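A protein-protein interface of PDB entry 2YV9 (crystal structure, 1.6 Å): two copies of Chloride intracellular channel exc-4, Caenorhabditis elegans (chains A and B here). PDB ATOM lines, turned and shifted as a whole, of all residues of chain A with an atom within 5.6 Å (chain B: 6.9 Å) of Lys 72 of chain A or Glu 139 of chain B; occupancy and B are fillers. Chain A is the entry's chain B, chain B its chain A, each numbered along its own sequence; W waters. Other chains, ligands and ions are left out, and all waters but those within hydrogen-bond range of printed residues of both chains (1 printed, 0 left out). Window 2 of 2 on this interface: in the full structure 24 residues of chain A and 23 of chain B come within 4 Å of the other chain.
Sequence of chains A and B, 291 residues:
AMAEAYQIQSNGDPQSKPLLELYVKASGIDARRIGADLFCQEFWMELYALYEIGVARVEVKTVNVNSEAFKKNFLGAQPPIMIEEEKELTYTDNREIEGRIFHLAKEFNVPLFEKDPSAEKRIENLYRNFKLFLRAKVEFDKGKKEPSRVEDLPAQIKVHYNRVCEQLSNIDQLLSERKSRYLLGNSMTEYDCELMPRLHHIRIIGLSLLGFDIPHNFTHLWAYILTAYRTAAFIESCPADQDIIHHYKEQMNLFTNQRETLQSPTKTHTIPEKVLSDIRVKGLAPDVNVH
The side-chain amide oxygen (OD1) of Asn 73 of chain A sits at hydrogen-bond distance from the guanidinium group (NH1) of Arg 135 of chain B, at 3.1 Å. The side-chain carboxylate (OE2) of Glu 139 of chain B lies within salt-bridge range of the side-chain amino group (NZ) of Lys 72 of chain A.
The guanidinium group of Arg 135 of chain B is in salt-bridge range of the side-chain carboxylate of Glu 139 of chain B, 2.7 Å away. O of Ala 69 of chain A lies within hydrogen-bond range of ND2 of Asn 73 of chain A.
Among the printed residues, merely in contact across the chains: Glu 68 of chain A with Asn 253 of chain B (3.6 Å), Lys 71 of chain A with Gln 251 of chain B (3.5 Å), Lys 72 of chain A with Arg 135 of chain B (3.6 Å), Lys 72 of chain A with Gln 251 of chain B (3.3 Å), Lys 72 of chain A with Met 252 of chain B (3.8 Å) and Leu 75 of chain A with Gln 251 of chain B (3.7 Å).
Of the printed residues of chain B, Lys 72 of chain A touches Arg 135, Glu 139, Gln 251 and Met 252. Glu 139 of chain B touches one residue of chain A. Of the printed residues of chain A, Asn 253 of chain B touches Glu 68 (3.6 Å). Of the printed residues of chain B, Lys 71 of chain A touches Gln 251. Printed residues of chain A within 4 Å of Arg 135 of chain B: Lys 72 and Asn 73. Printed residues of chain B within 4 Å of Asn 73 of chain A: Arg 135. Phe 74 of chain A touches none of the printed residues of chain B. The nearest printed residue of chain B that does not touch Lys 72 of chain A is Asn 253 of chain B (5.1 Å). The nearest printed residue of chain A that does not touch Glu 139 of chain B is Asn 73 of chain A (7.3 Å). The nearest printed residue of chain A that does not touch Met 252 of chain B is Leu 75 of chain A (4.3 Å).
Of the 9 printed residues of chain A, 5 touch a printed residue of chain B. Of the 17 printed residues of chain B, 5 touch a printed residue of chain A. Printed residues of chain B that touch a printed residue of chain A: Arg 135, Glu 139, Gln 251, Met 252 and Asn 253. Hydrophobic or aromatic side chains of chain B within 4 Å of the printed part of chain A: Met 252. Among the printed residues, Asp or Glu carboxylates within 4 Å of a Lys or Arg side-chain nitrogen of the other chain: Lys 72 of chain A with Glu 139 of chain B.
No position is printed for both chains. Of the 8 pairs that touch across the chains among the printed residues, none has its exchanged pair printed and touching as well.
Water W1 bridges the backbone carbonyl oxygen of Lys 72 of chain A (2.6 Å) and the guanidinium group of Arg 135 of chain B (3.0 Å).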
ATOM      1  N   SER A  67       5.414  33.528  11.672  1.00  0.00           N
ATOM      2  CA  SER A  67       6.826  33.500  11.281  1.00  0.00           C
ATOM      3  C   SER A  67       7.164  32.343  10.348  1.00  0.00           C
ATOM      4  O   SER A  67       6.540  31.280  10.396  1.00  0.00           O
ATOM      5  CB  SER A  67       7.708  33.421  12.517  1.00  0.00           C
ATOM      6  OG  SER A  67       7.583  32.157  13.121  1.00  0.00           O
ATOM      7  N   GLU A  68       8.176  32.545   9.509  1.00  0.00           N
ATOM      8  CA  GLU A  68       8.568  31.536   8.529  1.00  0.00           C
ATOM      9  C   GLU A  68       9.127  30.287   9.190  1.00  0.00           C
ATOM     10  O   GLU A  68       8.813  29.155   8.749  1.00  0.00           O
ATOM     11  CB  GLU A  68       9.598  32.097   7.526  1.00  0.00           C
ATOM     12  CG  GLU A  68       9.891  31.155   6.341  1.00  0.00           C
ATOM     13  CD  GLU A  68      11.273  31.369   5.711  1.00  0.00           C
ATOM     14  OE1 GLU A  68      12.202  31.821   6.420  1.00  0.00           O
ATOM     15  OE2 GLU A  68      11.427  31.069   4.504  1.00  0.00           O
ATOM     16  N   ALA A  69       9.962  30.470  10.211  1.00  0.00           N
ATOM     17  CA  ALA A  69      10.571  29.340  10.889  1.00  0.00           C
ATOM     18  C   ALA A  69       9.502  28.480  11.572  1.00  0.00           C
ATOM     19  O   ALA A  69       9.604  27.248  11.552  1.00  0.00           O
ATOM     20  CB  ALA A  69      11.616  29.794  11.908  1.00  0.00           C
ATOM     21  N   PHE A  70       8.480  29.126  12.140  1.00  0.00           N
ATOM     22  CA  PHE A  70       7.390  28.395  12.801  1.00  0.00           C
ATOM     23  C   PHE A  70       6.639  27.480  11.844  1.00  0.00           C
ATOM     24  O   PHE A  70       6.378  26.322  12.167  1.00  0.00           O
ATOM     25  CB  PHE A  70       6.378  29.325  13.493  1.00  0.00           C
ATOM     26  CG  PHE A  70       5.320  28.559  14.270  1.00  0.00           C
ATOM     27  CD1 PHE A  70       5.673  27.842  15.402  1.00  0.00           C
ATOM     28  CD2 PHE A  70       4.023  28.490  13.814  1.00  0.00           C
ATOM     29  CE1 PHE A  70       4.735  27.096  16.083  1.00  0.00           C
ATOM     30  CE2 PHE A  70       3.080  27.744  14.502  1.00  0.00           C
ATOM     31  CZ  PHE A  70       3.446  27.060  15.630  1.00  0.00           C
ATOM     32  N   LYS A  71       6.294  28.015  10.672  1.00  0.00           N
ATOM     33  CA  LYS A  71       5.549  27.287   9.663  1.00  0.00           C
ATOM     34  C   LYS A  71       6.337  26.093   9.179  1.00  0.00           C
ATOM     35  O   LYS A  71       5.786  24.994   8.994  1.00  0.00           O
ATOM     36  CB  LYS A  71       5.224  28.203   8.478  1.00  0.00           C
ATOM     37  CG  LYS A  71       4.282  29.350   8.801  1.00  0.00           C
ATOM     38  CD  LYS A  71       4.091  30.284   7.599  1.00  0.00           C
ATOM     39  CE  LYS A  71       3.143  31.441   7.916  1.00  0.00           C
ATOM     40  NZ  LYS A  71       3.251  32.573   6.932  1.00  0.00           N
ATOM     41  N   LYS A  72       7.638  26.291   8.976  1.00  0.00           N
ATOM     42  CA  LYS A  72       8.478  25.252   8.382  1.00  0.00           C
ATOM     43  C   LYS A  72       8.777  24.160   9.418  1.00  0.00           C
ATOM     44  O   LYS A  72       8.814  22.968   9.094  1.00  0.00           O
ATOM     45  CB  LYS A  72       9.776  25.873   7.816  1.00  0.00           C
ATOM     46  CG  LYS A  72      10.565  24.952   6.910  1.00  0.00           C
ATOM     47  CD  LYS A  72      11.534  25.717   5.983  1.00  0.00           C
ATOM     48  CE  LYS A  72      12.371  26.712   6.755  1.00  0.00           C
ATOM     49  NZ  LYS A  72      13.676  27.016   6.073  1.00  0.00           N
ATOM     50  N   ASN A  73       8.966  24.585  10.669  1.00  0.00           N
ATOM     51  CA  ASN A  73       9.279  23.660  11.771  1.00  0.00           C
ATOM     52  C   ASN A  73       8.118  22.762  12.191  1.00  0.00           C
ATOM     53  O   ASN A  73       8.358  21.646  12.642  1.00  0.00           O
ATOM     54  CB  ASN A  73       9.790  24.413  12.997  1.00  0.00           C
ATOM     55  CG  ASN A  73      11.195  24.976  12.808  1.00  0.00           C
ATOM     56  OD1 ASN A  73      12.108  24.282  12.355  1.00  0.00           O
ATOM     57  ND2 ASN A  73      11.378  26.231  13.189  1.00  0.00           N
ATOM     58  N   PHE A  74       6.881  23.231  12.026  1.00  0.00           N
ATOM     59  CA  PHE A  74       5.700  22.467  12.448  1.00  0.00           C
ATOM     60  C   PHE A  74       4.678  22.203  11.357  1.00  0.00           C
ATOM     61  O   PHE A  74       3.596  21.659  11.630  1.00  0.00           O
ATOM     62  CB  PHE A  74       5.070  23.123  13.676  1.00  0.00           C
ATOM     63  CG  PHE A  74       6.016  23.188  14.824  1.00  0.00           C
ATOM     64  CD1 PHE A  74       6.349  22.037  15.539  1.00  0.00           C
ATOM     65  CD2 PHE A  74       6.627  24.385  15.164  1.00  0.00           C
ATOM     66  CE1 PHE A  74       7.256  22.097  16.583  1.00  0.00           C
ATOM     67  CE2 PHE A  74       7.528  24.442  16.201  1.00  0.00           C
ATOM     68  CZ  PHE A  74       7.847  23.312  16.907  1.00  0.00           C
ATOM     69  N   LEU A  75       5.039  22.544  10.112  1.00  0.00           N
ATOM     70  CA  LEU A  75       4.237  22.238   8.955  1.00  0.00           C
ATOM     71  C   LEU A  75       2.772  22.627   9.126  1.00  0.00           C
ATOM     72  O   LEU A  75       1.868  21.853   8.796  1.00  0.00           O
ATOM     73  CB  LEU A  75       4.388  20.736   8.605  1.00  0.00           C
ATOM     74  CG  LEU A  75       5.817  20.372   8.177  1.00  0.00           C
ATOM     75  CD1 LEU A  75       6.006  18.909   7.775  1.00  0.00           C
ATOM     76  CD2 LEU A  75       6.204  21.255   7.004  1.00  0.00           C
ATOM     77  N   PHE B 133      13.038  13.847   6.996  1.00  0.00           N
ATOM     78  CA  PHE B 133      13.646  13.636   5.691  1.00  0.00           C
ATOM     79  C   PHE B 133      13.181  14.732   4.709  1.00  0.00           C
ATOM     80  O   PHE B 133      13.972  15.320   3.937  1.00  0.00           O
ATOM     81  CB  PHE B 133      13.278  12.276   5.102  1.00  0.00           C
ATOM     82  CG  PHE B 133      13.910  12.013   3.771  1.00  0.00           C
ATOM     83  CD1 PHE B 133      15.263  12.218   3.576  1.00  0.00           C
ATOM     84  CD2 PHE B 133      13.152  11.577   2.671  1.00  0.00           C
ATOM     85  CE1 PHE B 133      15.838  11.997   2.325  1.00  0.00           C
ATOM     86  CE2 PHE B 133      13.711  11.376   1.443  1.00  0.00           C
ATOM     87  CZ  PHE B 133      15.046  11.587   1.251  1.00  0.00           C
ATOM     88  N   LEU B 134      11.892  15.052   4.782  1.00  0.00           N
ATOM     89  CA  LEU B 134      11.337  16.120   3.936  1.00  0.00           C
ATOM     90  C   LEU B 134      12.118  17.391   4.174  1.00  0.00           C
ATOM     91  O   LEU B 134      12.589  18.040   3.224  1.00  0.00           O
ATOM     92  CB  LEU B 134       9.853  16.278   4.183  1.00  0.00           C
ATOM     93  CG  LEU B 134       9.176  17.493   3.569  1.00  0.00           C
ATOM     94  CD1 LEU B 134       9.155  17.419   2.043  1.00  0.00           C
ATOM     95  CD2 LEU B 134       7.784  17.592   4.209  1.00  0.00           C
ATOM     96  N   ARG B 135      12.252  17.783   5.430  1.00  0.00           N
ATOM     97  CA  ARG B 135      12.955  19.021   5.729  1.00  0.00           C
ATOM     98  C   ARG B 135      14.456  18.909   5.343  1.00  0.00           C
ATOM     99  O   ARG B 135      15.028  19.837   4.732  1.00  0.00           O
ATOM    100  CB  ARG B 135      12.809  19.367   7.202  1.00  0.00           C
ATOM    101  CG  ARG B 135      13.673  20.545   7.677  1.00  0.00           C
ATOM    102  CD  ARG B 135      13.155  21.846   7.046  1.00  0.00           C
ATOM    103  NE  ARG B 135      13.774  23.068   7.571  1.00  0.00           N
ATOM    104  CZ  ARG B 135      13.518  23.581   8.771  1.00  0.00           C
ATOM    105  NH1 ARG B 135      12.730  22.965   9.623  1.00  0.00           N
ATOM    106  NH2 ARG B 135      14.117  24.709   9.153  1.00  0.00           N
ATOM    107  N   ALA B 136      15.111  17.785   5.667  1.00  0.00           N
ATOM    108  CA  ALA B 136      16.558  17.660   5.378  1.00  0.00           C
ATOM    109  C   ALA B 136      16.813  17.700   3.871  1.00  0.00           C
ATOM    110  O   ALA B 136      17.748  18.374   3.414  1.00  0.00           O
ATOM    111  CB  ALA B 136      17.081  16.362   5.947  1.00  0.00           C
ATOM    112  N   LYS B 137      16.000  17.009   3.080  1.00  0.00           N
ATOM    113  CA  LYS B 137      16.284  16.947   1.657  1.00  0.00           C
ATOM    114  C   LYS B 137      15.978  18.286   0.976  1.00  0.00           C
ATOM    115  O   LYS B 137      16.747  18.773   0.092  1.00  0.00           O
ATOM    116  CB  LYS B 137      15.543  15.827   0.934  1.00  0.00           C
ATOM    117  CG  LYS B 137      16.240  15.518  -0.388  1.00  0.00           C
ATOM    118  CD  LYS B 137      15.375  14.676  -1.277  1.00  0.00           C
ATOM    119  CE  LYS B 137      16.136  14.273  -2.501  1.00  0.00           C
ATOM    120  NZ  LYS B 137      16.078  15.321  -3.507  1.00  0.00           N
ATOM    121  N   VAL B 138      14.880  18.884   1.420  1.00  0.00           N
ATOM    122  CA  VAL B 138      14.498  20.229   0.859  1.00  0.00           C
ATOM    123  C   VAL B 138      15.597  21.246   1.091  1.00  0.00           C
ATOM    124  O   VAL B 138      15.941  22.059   0.210  1.00  0.00           O
ATOM    125  CB  VAL B 138      13.145  20.742   1.432  1.00  0.00           C
ATOM    126  CG1 VAL B 138      12.966  22.260   1.235  1.00  0.00           C
ATOM    127  CG2 VAL B 138      12.003  19.956   0.777  1.00  0.00           C
ATOM    128  N   GLU B 139      16.162  21.235   2.284  1.00  0.00           N
ATOM    129  CA  GLU B 139      17.249  22.182   2.600  1.00  0.00           C
ATOM    130  C   GLU B 139      18.542  21.803   1.844  1.00  0.00           C
ATOM    131  O   GLU B 139      19.333  22.669   1.409  1.00  0.00           O
ATOM    132  CB  GLU B 139      17.510  22.231   4.102  1.00  0.00           C
ATOM    133  CG  GLU B 139      16.309  22.660   4.931  1.00  0.00           C
ATOM    134  CD  GLU B 139      16.015  24.174   4.953  1.00  0.00           C
ATOM    135  OE1 GLU B 139      16.708  24.976   4.276  1.00  0.00           O
ATOM    136  OE2 GLU B 139      15.085  24.558   5.710  1.00  0.00           O
ATOM    137  N   PHE B 140      18.769  20.514   1.670  1.00  0.00           N
ATOM    138  CA  PHE B 140      19.964  20.072   0.954  1.00  0.00           C
ATOM    139  C   PHE B 140      19.908  20.501  -0.504  1.00  0.00           C
ATOM    140  O   PHE B 140      20.944  20.845  -1.131  1.00  0.00           O
ATOM    141  CB  PHE B 140      20.074  18.543   1.022  1.00  0.00           C
ATOM    142  CG  PHE B 140      21.324  18.022   0.441  1.00  0.00           C
ATOM    143  CD1 PHE B 140      22.546  18.294   1.058  1.00  0.00           C
ATOM    144  CD2 PHE B 140      21.320  17.299  -0.734  1.00  0.00           C
ATOM    145  CE1 PHE B 140      23.725  17.819   0.511  1.00  0.00           C
ATOM    146  CE2 PHE B 140      22.490  16.821  -1.272  1.00  0.00           C
ATOM    147  CZ  PHE B 140      23.692  17.088  -0.657  1.00  0.00           C
ATOM    148  N   ASP B 141      18.697  20.528  -1.046  1.00  0.00           N
ATOM    149  CA  ASP B 141      18.489  20.783  -2.481  1.00  0.00           C
ATOM    150  C   ASP B 141      18.350  22.279  -2.777  1.00  0.00           C
ATOM    151  O   ASP B 141      18.252  22.670  -3.927  1.00  0.00           O
ATOM    152  CB  ASP B 141      17.269  20.036  -3.006  1.00  0.00           C
ATOM    153  CG  ASP B 141      17.501  18.526  -3.116  1.00  0.00           C
ATOM    154  OD1 ASP B 141      18.685  18.134  -3.235  1.00  0.00           O
ATOM    155  OD2 ASP B 141      16.498  17.762  -3.158  1.00  0.00           O
ATOM    156  N   LYS B 142      18.345  23.098  -1.737  1.00  0.00           N
ATOM    157  CA  LYS B 142      18.247  24.565  -1.881  1.00  0.00           C
ATOM    158  C   LYS B 142      19.440  25.044  -2.722  1.00  0.00           C
ATOM    159  O   LYS B 142      20.586  24.714  -2.435  1.00  0.00           O
ATOM    160  CB  LYS B 142      18.235  25.228  -0.495  1.00  0.00           C
ATOM    161  CG  LYS B 142      17.741  26.653  -0.437  1.00  0.00           C
ATOM    162  CD  LYS B 142      17.637  27.128   1.022  1.00  0.00           C
ATOM    163  CE  LYS B 142      17.493  28.658   1.127  1.00  0.00           C
ATOM    164  NZ  LYS B 142      16.092  29.155   1.237  1.00  0.00           N
ATOM    165  N   GLY B 143      19.166  25.807  -3.781  1.00  0.00           N
ATOM    166  CA  GLY B 143      20.235  26.331  -4.641  1.00  0.00           C
ATOM    167  C   GLY B 143      20.733  25.375  -5.704  1.00  0.00           C
ATOM    168  O   GLY B 143      21.820  25.541  -6.251  1.00  0.00           O
ATOM    169  N   LYS B 144      19.926  24.373  -6.007  1.00  0.00           N
ATOM    170  CA  LYS B 144      20.211  23.435  -7.072  1.00  0.00           C
ATOM    171  C   LYS B 144      19.059  23.474  -8.046  1.00  0.00           C
ATOM    172  O   LYS B 144      17.911  23.505  -7.625  1.00  0.00           O
ATOM    173  CB  LYS B 144      20.271  22.015  -6.500  1.00  0.00           C
ATOM    174  CG  LYS B 144      21.402  21.784  -5.530  1.00  0.00           C
ATOM    175  CD  LYS B 144      21.367  20.354  -5.002  1.00  0.00           C
ATOM    176  CE  LYS B 144      22.584  20.011  -4.130  1.00  0.00           C
ATOM    177  NZ  LYS B 144      22.722  20.871  -2.930  1.00  0.00           N
ATOM    178  N   ILE B 157      21.797  13.126   5.713  1.00  0.00           N
ATOM    179  CA  ILE B 157      20.489  13.334   5.110  1.00  0.00           C
ATOM    180  C   ILE B 157      19.808  11.985   4.825  1.00  0.00           C
ATOM    181  O   ILE B 157      18.625  11.808   5.104  1.00  0.00           O
ATOM    182  CB  ILE B 157      20.597  14.170   3.863  1.00  0.00           C
ATOM    183  CG1 ILE B 157      21.266  15.501   4.236  1.00  0.00           C
ATOM    184  CG2 ILE B 157      19.205  14.464   3.239  1.00  0.00           C
ATOM    185  CD1 ILE B 157      21.621  16.191   3.147  1.00  0.00           C
ATOM    186  N   GLN B 251       4.108  25.247   3.344  1.00  0.00           N
ATOM    187  CA  GLN B 251       4.773  25.281   4.664  1.00  0.00           C
ATOM    188  C   GLN B 251       6.324  25.129   4.610  1.00  0.00           C
ATOM    189  O   GLN B 251       7.011  25.699   5.451  1.00  0.00           O
ATOM    190  CB  GLN B 251       4.198  24.207   5.611  1.00  0.00           C
ATOM    191  CG  GLN B 251       2.652  24.189   5.780  1.00  0.00           C
ATOM    192  CD  GLN B 251       2.059  25.398   6.520  1.00  0.00           C
ATOM    193  OE1 GLN B 251       2.736  26.090   7.288  1.00  0.00           O
ATOM    194  NE2 GLN B 251       0.762  25.628   6.305  1.00  0.00           N
ATOM    195  N   MET B 252       6.825  24.316   3.668  1.00  0.00           N
ATOM    196  CA  MET B 252       8.272  24.146   3.402  1.00  0.00           C
ATOM    197  C   MET B 252       8.787  25.361   2.557  1.00  0.00           C
ATOM    198  O   MET B 252       9.923  25.336   2.071  1.00  0.00           O
ATOM    199  CB  MET B 252       8.571  22.783   2.666  1.00  0.00           C
ATOM    200  CG  MET B 252       8.703  21.386   3.514  1.00  0.00           C
ATOM    201  SD  MET B 252      10.092  21.472   4.688  1.00  0.00           S
ATOM    202  CE  MET B 252      11.230  22.603   3.898  1.00  0.00           C
ATOM    203  N   ASN B 253       7.959  26.406   2.379  1.00  0.00           N
ATOM    204  CA  ASN B 253       8.262  27.521   1.471  1.00  0.00           C
ATOM    205  C   ASN B 253       9.028  27.087   0.223  1.00  0.00           C
ATOM    206  O   ASN B 253      10.194  27.420   0.065  1.00  0.00           O
ATOM    207  CB  ASN B 253       9.010  28.627   2.216  1.00  0.00           C
ATOM    208  CG  ASN B 253       8.073  29.533   2.985  1.00  0.00           C
ATOM    209  OD1 ASN B 253       7.735  29.270   4.147  1.00  0.00           O
ATOM    210  ND2 ASN B 253       7.647  30.619   2.336  1.00  0.00           N
ATOM    211  N   LEU B 254       8.373  26.286  -0.613  1.00  0.00           N
ATOM    212  CA  LEU B 254       8.882  25.905  -1.944  1.00  0.00           C
ATOM    213  C   LEU B 254       7.935  26.421  -3.020  1.00  0.00           C
ATOM    214  O   LEU B 254       6.711  26.566  -2.790  1.00  0.00           O
ATOM    215  CB  LEU B 254       9.017  24.400  -2.117  1.00  0.00           C
ATOM    216  CG  LEU B 254       9.665  23.610  -1.005  1.00  0.00           C
ATOM    217  CD1 LEU B 254       9.586  22.113  -1.321  1.00  0.00           C
ATOM    218  CD2 LEU B 254      11.100  24.065  -0.828  1.00  0.00           C
HETATM  219  O   HOH W   1      10.487  21.041   9.395  1.00  0.00           O
